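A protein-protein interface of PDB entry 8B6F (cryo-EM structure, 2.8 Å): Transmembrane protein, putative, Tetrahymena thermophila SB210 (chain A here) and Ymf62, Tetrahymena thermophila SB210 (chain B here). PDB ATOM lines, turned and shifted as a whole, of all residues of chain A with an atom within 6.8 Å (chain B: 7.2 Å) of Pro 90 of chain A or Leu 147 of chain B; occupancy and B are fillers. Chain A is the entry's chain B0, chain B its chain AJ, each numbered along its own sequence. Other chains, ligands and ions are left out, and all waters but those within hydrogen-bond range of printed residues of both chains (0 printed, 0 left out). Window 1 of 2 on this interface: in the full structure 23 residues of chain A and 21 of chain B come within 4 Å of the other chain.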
ATOM      1  N   TYR A  69      -2.254  19.881  28.061  1.00  0.00           N
ATOM      2  CA  TYR A  69      -1.828  19.021  26.964  1.00  0.00           C
ATOM      3  C   TYR A  69      -2.960  18.193  26.384  1.00  0.00           C
ATOM      4  O   TYR A  69      -3.127  18.156  25.159  1.00  0.00           O
ATOM      5  CB  TYR A  69      -0.693  18.096  27.434  1.00  0.00           C
ATOM      6  CG  TYR A  69       0.625  18.811  27.615  1.00  0.00           C
ATOM      7  CD1 TYR A  69       1.519  18.930  26.561  1.00  0.00           C
ATOM      8  CD2 TYR A  69       0.969  19.378  28.834  1.00  0.00           C
ATOM      9  CE1 TYR A  69       2.721  19.587  26.715  1.00  0.00           C
ATOM     10  CE2 TYR A  69       2.169  20.038  28.998  1.00  0.00           C
ATOM     11  CZ  TYR A  69       3.041  20.139  27.934  1.00  0.00           C
ATOM     12  OH  TYR A  69       4.239  20.794  28.090  1.00  0.00           O
ATOM     13  N   ALA A  73      -4.430  18.526  22.578  1.00  0.00           N
ATOM     14  CA  ALA A  73      -4.126  17.347  21.776  1.00  0.00           C
ATOM     15  C   ALA A  73      -5.386  16.768  21.147  1.00  0.00           C
ATOM     16  O   ALA A  73      -5.376  16.362  19.979  1.00  0.00           O
ATOM     17  CB  ALA A  73      -3.426  16.296  22.636  1.00  0.00           C
ATOM     18  N   TRP A  76      -7.000  19.226  18.556  1.00  0.00           N
ATOM     19  CA  TRP A  76      -6.064  19.690  17.544  1.00  0.00           C
ATOM     20  C   TRP A  76      -6.696  19.672  16.160  1.00  0.00           C
ATOM     21  O   TRP A  76      -7.440  18.753  15.807  1.00  0.00           O
ATOM     22  CB  TRP A  76      -4.813  18.816  17.553  1.00  0.00           C
ATOM     23  CG  TRP A  76      -3.820  19.176  16.495  1.00  0.00           C
ATOM     24  CD1 TRP A  76      -2.947  20.221  16.513  1.00  0.00           C
ATOM     25  CD2 TRP A  76      -3.595  18.484  15.262  1.00  0.00           C
ATOM     26  NE1 TRP A  76      -2.191  20.225  15.367  1.00  0.00           N
ATOM     27  CE2 TRP A  76      -2.570  19.168  14.582  1.00  0.00           C
ATOM     28  CE3 TRP A  76      -4.161  17.353  14.667  1.00  0.00           C
ATOM     29  CZ2 TRP A  76      -2.099  18.760  13.336  1.00  0.00           C
ATOM     30  CZ3 TRP A  76      -3.693  16.948  13.430  1.00  0.00           C
ATOM     31  CH2 TRP A  76      -2.672  17.651  12.778  1.00  0.00           C
ATOM     32  N   ASN A  81      -2.166  25.086  14.537  1.00  0.00           N
ATOM     33  CA  ASN A  81      -0.773  25.379  14.836  1.00  0.00           C
ATOM     34  C   ASN A  81      -0.353  26.696  14.200  1.00  0.00           C
ATOM     35  O   ASN A  81      -0.745  27.017  13.076  1.00  0.00           O
ATOM     36  CB  ASN A  81       0.127  24.248  14.343  1.00  0.00           C
ATOM     37  CG  ASN A  81      -0.153  22.940  15.045  1.00  0.00           C
ATOM     38  OD1 ASN A  81      -0.898  22.100  14.543  1.00  0.00           O
ATOM     39  ND2 ASN A  81       0.440  22.761  16.220  1.00  0.00           N
ATOM     40  N   ASN A  87       5.165  27.064  19.027  1.00  0.00           N
ATOM     41  CA  ASN A  87       4.252  26.166  19.715  1.00  0.00           C
ATOM     42  C   ASN A  87       4.767  25.849  21.117  1.00  0.00           C
ATOM     43  O   ASN A  87       5.906  26.148  21.476  1.00  0.00           O
ATOM     44  CB  ASN A  87       4.070  24.878  18.913  1.00  0.00           C
ATOM     45  CG  ASN A  87       3.532  25.134  17.521  1.00  0.00           C
ATOM     46  OD1 ASN A  87       2.321  25.220  17.318  1.00  0.00           O
ATOM     47  ND2 ASN A  87       4.432  25.254  16.551  1.00  0.00           N
ATOM     48  N   THR A  88       3.900  25.235  21.916  1.00  0.00           N
ATOM     49  CA  THR A  88       4.287  24.820  23.255  1.00  0.00           C
ATOM     50  C   THR A  88       5.345  23.728  23.177  1.00  0.00           C
ATOM     51  O   THR A  88       5.331  22.890  22.272  1.00  0.00           O
ATOM     52  CB  THR A  88       3.071  24.318  24.034  1.00  0.00           C
ATOM     53  OG1 THR A  88       2.513  23.172  23.378  1.00  0.00           O
ATOM     54  CG2 THR A  88       2.011  25.406  24.132  1.00  0.00           C
ATOM     55  N   ARG A  89       6.267  23.746  24.128  1.00  0.00           N
ATOM     56  CA  ARG A  89       7.342  22.769  24.133  1.00  0.00           C
ATOM     57  C   ARG A  89       6.830  21.418  24.633  1.00  0.00           C
ATOM     58  O   ARG A  89       5.845  21.356  25.372  1.00  0.00           O
ATOM     59  CB  ARG A  89       8.486  23.243  25.021  1.00  0.00           C
ATOM     60  CG  ARG A  89       8.924  24.679  24.767  1.00  0.00           C
ATOM     61  CD  ARG A  89       9.432  24.870  23.353  1.00  0.00           C
ATOM     62  NE  ARG A  89       9.959  26.214  23.144  1.00  0.00           N
ATOM     63  CZ  ARG A  89       9.259  27.241  22.681  1.00  0.00           C
ATOM     64  NH1 ARG A  89       7.980  27.123  22.363  1.00  0.00           N
ATOM     65  NH2 ARG A  89       9.860  28.416  22.523  1.00  0.00           N
ATOM     66  N   PRO A  90       7.479  20.319  24.244  1.00  0.00           N
ATOM     67  CA  PRO A  90       7.052  19.006  24.742  1.00  0.00           C
ATOM     68  C   PRO A  90       7.171  18.922  26.255  1.00  0.00           C
ATOM     69  O   PRO A  90       8.042  19.539  26.868  1.00  0.00           O
ATOM     70  CB  PRO A  90       8.017  18.031  24.055  1.00  0.00           C
ATOM     71  CG  PRO A  90       8.538  18.763  22.879  1.00  0.00           C
ATOM     72  CD  PRO A  90       8.579  20.206  23.272  1.00  0.00           C
ATOM     73  N   LEU A  91       6.275  18.139  26.858  1.00  0.00           N
ATOM     74  CA  LEU A  91       6.319  17.962  28.306  1.00  0.00           C
ATOM     75  C   LEU A  91       7.652  17.366  28.742  1.00  0.00           C
ATOM     76  O   LEU A  91       8.253  17.823  29.720  1.00  0.00           O
ATOM     77  CB  LEU A  91       5.155  17.082  28.763  1.00  0.00           C
ATOM     78  CG  LEU A  91       4.986  16.903  30.275  1.00  0.00           C
ATOM     79  CD1 LEU A  91       4.849  18.243  30.983  1.00  0.00           C
ATOM     80  CD2 LEU A  91       3.782  16.026  30.570  1.00  0.00           C
ATOM     81  N   LEU A  92       8.127  16.349  28.030  1.00  0.00           N
ATOM     82  CA  LEU A  92       9.467  15.800  28.214  1.00  0.00           C
ATOM     83  C   LEU A  92      10.291  16.228  27.006  1.00  0.00           C
ATOM     84  O   LEU A  92      10.223  15.605  25.944  1.00  0.00           O
ATOM     85  CB  LEU A  92       9.429  14.282  28.359  1.00  0.00           C
ATOM     86  CG  LEU A  92       8.811  13.729  29.646  1.00  0.00           C
ATOM     87  CD1 LEU A  92       8.724  12.214  29.587  1.00  0.00           C
ATOM     88  CD2 LEU A  92       9.610  14.163  30.863  1.00  0.00           C
ATOM     89  N   ARG A  93      11.071  17.292  27.174  1.00  0.00           N
ATOM     90  CA  ARG A  93      11.800  17.871  26.056  1.00  0.00           C
ATOM     91  C   ARG A  93      12.908  16.939  25.589  1.00  0.00           C
ATOM     92  O   ARG A  93      13.698  16.441  26.395  1.00  0.00           O
ATOM     93  CB  ARG A  93      12.385  19.223  26.448  1.00  0.00           C
ATOM     94  CG  ARG A  93      11.330  20.265  26.761  1.00  0.00           C
ATOM     95  CD  ARG A  93      11.865  21.665  26.562  1.00  0.00           C
ATOM     96  NE  ARG A  93      12.286  21.890  25.184  1.00  0.00           N
ATOM     97  CZ  ARG A  93      12.677  23.060  24.699  1.00  0.00           C
ATOM     98  NH1 ARG A  93      12.699  24.148  25.450  1.00  0.00           N
ATOM     99  NH2 ARG A  93      13.057  23.140  23.428  1.00  0.00           N
ATOM    100  N   TYR A  94      12.971  16.718  24.281  1.00  0.00           N
ATOM    101  CA  TYR A  94      13.986  15.860  23.688  1.00  0.00           C
ATOM    102  C   TYR A  94      14.792  16.632  22.651  1.00  0.00           C
ATOM    103  O   TYR A  94      15.223  16.075  21.644  1.00  0.00           O
ATOM    104  CB  TYR A  94      13.340  14.632  23.045  1.00  0.00           C
ATOM    105  CG  TYR A  94      12.274  14.965  22.028  1.00  0.00           C
ATOM    106  CD1 TYR A  94      10.958  15.179  22.416  1.00  0.00           C
ATOM    107  CD2 TYR A  94      12.583  15.061  20.679  1.00  0.00           C
ATOM    108  CE1 TYR A  94       9.980  15.481  21.490  1.00  0.00           C
ATOM    109  CE2 TYR A  94      11.614  15.363  19.745  1.00  0.00           C
ATOM    110  CZ  TYR A  94      10.314  15.572  20.157  1.00  0.00           C
ATOM    111  OH  TYR A  94       9.345  15.875  19.230  1.00  0.00           O
ATOM    112  N   PHE B  32      13.971  25.800  18.133  1.00  0.00           N
ATOM    113  CA  PHE B  32      13.518  26.575  19.276  1.00  0.00           C
ATOM    114  C   PHE B  32      14.605  27.559  19.686  1.00  0.00           C
ATOM    115  O   PHE B  32      15.800  27.275  19.567  1.00  0.00           O
ATOM    116  CB  PHE B  32      13.162  25.668  20.459  1.00  0.00           C
ATOM    117  CG  PHE B  32      11.815  25.010  20.342  1.00  0.00           C
ATOM    118  CD1 PHE B  32      10.693  25.746  20.006  1.00  0.00           C
ATOM    119  CD2 PHE B  32      11.672  23.655  20.580  1.00  0.00           C
ATOM    120  CE1 PHE B  32       9.457  25.145  19.906  1.00  0.00           C
ATOM    121  CE2 PHE B  32      10.437  23.047  20.482  1.00  0.00           C
ATOM    122  CZ  PHE B  32       9.328  23.793  20.144  1.00  0.00           C
ATOM    123  N   GLN B  77      16.304  18.168  31.536  1.00  0.00           N
ATOM    124  CA  GLN B  77      15.700  17.746  32.797  1.00  0.00           C
ATOM    125  C   GLN B  77      16.571  16.785  33.594  1.00  0.00           C
ATOM    126  O   GLN B  77      16.048  16.002  34.391  1.00  0.00           O
ATOM    127  CB  GLN B  77      14.322  17.120  32.562  1.00  0.00           C
ATOM    128  CG  GLN B  77      13.395  18.007  31.742  1.00  0.00           C
ATOM    129  CD  GLN B  77      12.067  17.349  31.438  1.00  0.00           C
ATOM    130  OE1 GLN B  77      11.845  16.186  31.768  1.00  0.00           O
ATOM    131  NE2 GLN B  77      11.171  18.097  30.807  1.00  0.00           N
ATOM    132  N   GLU B 142      12.352  18.484  17.469  1.00  0.00           N
ATOM    133  CA  GLU B 142      11.085  19.041  17.909  1.00  0.00           C
ATOM    134  C   GLU B 142      10.573  20.010  16.850  1.00  0.00           C
ATOM    135  O   GLU B 142      11.353  20.680  16.167  1.00  0.00           O
ATOM    136  CB  GLU B 142      11.247  19.748  19.254  1.00  0.00           C
ATOM    137  CG  GLU B 142      11.696  18.827  20.381  1.00  0.00           C
ATOM    138  CD  GLU B 142      12.045  19.580  21.650  1.00  0.00           C
ATOM    139  OE1 GLU B 142      12.004  20.826  21.636  1.00  0.00           O
ATOM    140  OE2 GLU B 142      12.364  18.926  22.663  1.00  0.00           O
ATOM    141  N   LEU B 143       9.254  20.074  16.708  1.00  0.00           N
ATOM    142  CA  LEU B 143       8.547  20.790  15.649  1.00  0.00           C
ATOM    143  C   LEU B 143       8.546  19.985  14.356  1.00  0.00           C
ATOM    144  O   LEU B 143       7.972  20.444  13.363  1.00  0.00           O
ATOM    145  CB  LEU B 143       9.134  22.182  15.360  1.00  0.00           C
ATOM    146  CG  LEU B 143       9.245  23.124  16.557  1.00  0.00           C
ATOM    147  CD1 LEU B 143      10.124  24.311  16.223  1.00  0.00           C
ATOM    148  CD2 LEU B 143       7.862  23.580  16.990  1.00  0.00           C
ATOM    149  N   LEU B 145       6.896  17.220  13.926  1.00  0.00           N
ATOM    150  CA  LEU B 145       5.468  16.959  13.876  1.00  0.00           C
ATOM    151  C   LEU B 145       4.782  17.775  14.956  1.00  0.00           C
ATOM    152  O   LEU B 145       5.415  18.175  15.939  1.00  0.00           O
ATOM    153  CB  LEU B 145       5.154  15.469  14.077  1.00  0.00           C
ATOM    154  CG  LEU B 145       5.340  14.541  12.877  1.00  0.00           C
ATOM    155  CD1 LEU B 145       5.072  13.104  13.276  1.00  0.00           C
ATOM    156  CD2 LEU B 145       4.427  14.947  11.731  1.00  0.00           C
ATOM    157  N   PRO B 146       3.488  18.048  14.804  1.00  0.00           N
ATOM    158  CA  PRO B 146       2.778  18.805  15.840  1.00  0.00           C
ATOM    159  C   PRO B 146       2.852  18.098  17.185  1.00  0.00           C
ATOM    160  O   PRO B 146       2.796  16.870  17.267  1.00  0.00           O
ATOM    161  CB  PRO B 146       1.340  18.869  15.315  1.00  0.00           C
ATOM    162  CG  PRO B 146       1.461  18.669  13.848  1.00  0.00           C
ATOM    163  CD  PRO B 146       2.619  17.743  13.654  1.00  0.00           C
ATOM    164  N   LEU B 147       2.986  18.893  18.248  1.00  0.00           N
ATOM    165  CA  LEU B 147       3.029  18.328  19.589  1.00  0.00           C
ATOM    166  C   LEU B 147       1.732  17.623  19.955  1.00  0.00           C
ATOM    167  O   LEU B 147       1.731  16.777  20.853  1.00  0.00           O
ATOM    168  CB  LEU B 147       3.327  19.429  20.610  1.00  0.00           C
ATOM    169  CG  LEU B 147       3.351  19.003  22.079  1.00  0.00           C
ATOM    170  CD1 LEU B 147       4.449  17.983  22.332  1.00  0.00           C
ATOM    171  CD2 LEU B 147       3.524  20.211  22.976  1.00  0.00           C
ATOM    172  N   GLU B 148       0.630  17.952  19.279  1.00  0.00           N
ATOM    173  CA  GLU B 148      -0.660  17.374  19.629  1.00  0.00           C
ATOM    174  C   GLU B 148      -0.775  15.914  19.213  1.00  0.00           C
ATOM    175  O   GLU B 148      -1.684  15.222  19.682  1.00  0.00           O
ATOM    176  CB  GLU B 148      -1.781  18.193  18.992  1.00  0.00           C
ATOM    177  CG  GLU B 148      -1.975  19.568  19.626  1.00  0.00           C
ATOM    178  CD  GLU B 148      -0.860  20.534  19.291  1.00  0.00           C
ATOM    179  OE1 GLU B 148       0.105  20.120  18.618  1.00  0.00           O
ATOM    180  OE2 GLU B 148      -0.951  21.712  19.695  1.00  0.00           O
ATOM    181  N   LEU B 149       0.115  15.434  18.345  1.00  0.00           N
ATOM    182  CA  LEU B 149       0.109  14.023  17.982  1.00  0.00           C
ATOM    183  C   LEU B 149       0.715  13.152  19.073  1.00  0.00           C
ATOM    184  O   LEU B 149       0.311  11.995  19.232  1.00  0.00           O
ATOM    185  CB  LEU B 149       0.859  13.812  16.666  1.00  0.00           C
ATOM    186  CG  LEU B 149       0.299  14.534  15.438  1.00  0.00           C
ATOM    187  CD1 LEU B 149       1.106  14.173  14.204  1.00  0.00           C
ATOM    188  CD2 LEU B 149      -1.170  14.217  15.220  1.00  0.00           C
ATOM    189  N   SER B 150       1.679  13.677  19.826  1.00  0.00           N
ATOM    190  CA  SER B 150       2.285  12.929  20.917  1.00  0.00           C
ATOM    191  C   SER B 150       1.339  12.904  22.111  1.00  0.00           C
ATOM    192  O   SER B 150       0.791  13.938  22.501  1.00  0.00           O
ATOM    193  CB  SER B 150       3.622  13.557  21.310  1.00  0.00           C
ATOM    194  OG  SER B 150       4.237  12.830  22.359  1.00  0.00           O
ATOM    195  N   PHE B 151       1.151  11.717  22.692  1.00  0.00           N
ATOM    196  CA  PHE B 151       0.199  11.547  23.783  1.00  0.00           C
ATOM    197  C   PHE B 151       0.716  10.724  24.952  1.00  0.00           C
ATOM    198  O   PHE B 151       0.056  10.705  25.995  1.00  0.00           O
ATOM    199  CB  PHE B 151      -1.084  10.889  23.258  1.00  0.00           C
ATOM    200  CG  PHE B 151      -0.857   9.551  22.618  1.00  0.00           C
ATOM    201  CD1 PHE B 151      -0.505   9.461  21.282  1.00  0.00           C
ATOM    202  CD2 PHE B 151      -0.992   8.384  23.351  1.00  0.00           C
ATOM    203  CE1 PHE B 151      -0.292   8.233  20.688  1.00  0.00           C
ATOM    204  CE2 PHE B 151      -0.779   7.151  22.760  1.00  0.00           C
ATOM    205  CZ  PHE B 151      -0.430   7.077  21.428  1.00  0.00           C
ATOM    206  N   ASP B 153       3.195  11.039  27.049  1.00  0.00           N
ATOM    207  CA  ASP B 153       3.617  11.763  28.243  1.00  0.00           C
ATOM    208  C   ASP B 153       2.459  12.040  29.192  1.00  0.00           C
ATOM    209  O   ASP B 153       2.691  12.253  30.387  1.00  0.00           O
ATOM    210  CB  ASP B 153       4.289  13.080  27.848  1.00  0.00           C
ATOM    211  CG  ASP B 153       5.589  12.868  27.100  1.00  0.00           C
ATOM    212  OD1 ASP B 153       6.245  11.831  27.328  1.00  0.00           O
ATOM    213  OD2 ASP B 153       5.955  13.737  26.282  1.00  0.00           O
ATOM    214  N   ILE B 154       1.222  12.047  28.693  1.00  0.00           N
ATOM    215  CA  ILE B 154       0.071  12.260  29.563  1.00  0.00           C
ATOM    216  C   ILE B 154      -0.308  10.991  30.317  1.00  0.00           C
ATOM    217  O   ILE B 154      -0.992  11.070  31.344  1.00  0.00           O
ATOM    218  CB  ILE B 154      -1.133  12.780  28.754  1.00  0.00           C
ATOM    219  CG1 ILE B 154      -0.837  14.147  28.126  1.00  0.00           C
ATOM    220  CG2 ILE B 154      -2.382  12.894  29.623  1.00  0.00           C
ATOM    221  CD1 ILE B 154      -0.002  14.112  26.854  1.00  0.00           C
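Along chain A the printed residues that touch a printed residue of chain B span positions 69 to 94. Of the 13 printed residues of chain B, 8 touch a printed residue of chain A. Among the printed residues, Asp or Glu carboxylates within 4 Å of a Lys or Arg side-chain nitrogen of the other chain: Arg 93 of chain A with Glu 142 of chain B (3.1 Å).
The backbone carbonyl oxygen (O) of Leu 91 of chain A is in hydrogen-bond range of the side-chain amide nitrogen (NE2) of Gln 77 of chain B (3.1 Å). The side-chain carboxylate (OE1) of Glu 142 of chain B lies within salt-bridge range of the guanidinium group (NH2) of Arg 93 of chain A, 3.1 Å away. OE2 of Glu 142 of chain B is in hydrogen-bond range of N of Tyr 94 of chain A, at 2.8 Å.
Of the printed residues of chain B, Ala 73 of chain A touches Glu 148. Printed residues of chain B within 4 Å of Asn 81 of chain A: Glu 148 (3.6 Å). Of the printed residues of chain B, Asn 87 of chain A touches Leu 143 (3.8 Å). Of chain B, only Glu 142 (3.8 Å) and Leu 147 (3.7 Å) come within 4 Å of Pro 90 of chain A. Printed residues of chain A within 4 Å of Phe 32 of chain B: Arg 89 (3.3 Å) and Arg 93 (3.2 Å). Ser 150 of chain B touches none of the printed residues of chain A. Of the printed residues of chain A, Asp 153 of chain B touches Leu 91 (3.9 Å) and Leu 92 (3.4 Å). Ile 154 of chain B touches none of the printed residues of chain A. The nearest printed residue of chain B that does not touch Arg 93 of chain A is Asp 153 of chain B (6.3 Å).
O of Arg 89 of chain A is in hydrogen-bond range of OH of Tyr 69 of chain A. OD1 of Asn 81 of chain A sits at hydrogen-bond distance from NE1 of Trp 76 of chain A, 2.4 Å away. ND2 of Asn 81 of chain A lies within hydrogen-bond range of OD1 of Asn 87 of chain A (3.3 Å). NH1 of Arg 89 of chain A is in hydrogen-bond range of O of Asn 87 of chain A (2.5 Å).
CE1 of Tyr 69 of chain A touches CD2 of Leu 147 of chain B (3.9 Å). Ala 73 of chain A touches Glu 148 of chain B (CB to O, 3.6 Å). Trp 76 of chain A touches Pro 146 of chain B. Trp 76 of chain A touches Glu 148 of chain B. Asn 81 of chain A touches Glu 148 of chain B (ND2 to OE1, 3.6 Å). Asn 87 of chain A touches Leu 143 of chain B (ND2 to CD2, 3.8 Å). Phe 32 of chain B touches Arg 89 of chain A. Leu 92 of chain A touches Gln 77 of chain B (CD2 to OE1, 3.1 Å). CD1 of Leu 92 of chain A touches OD1 of Asp 153 of chain B, at 3.4 Å. N of Arg 93 of chain A touches NE2 of Gln 77 of chain B (3.7 Å).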
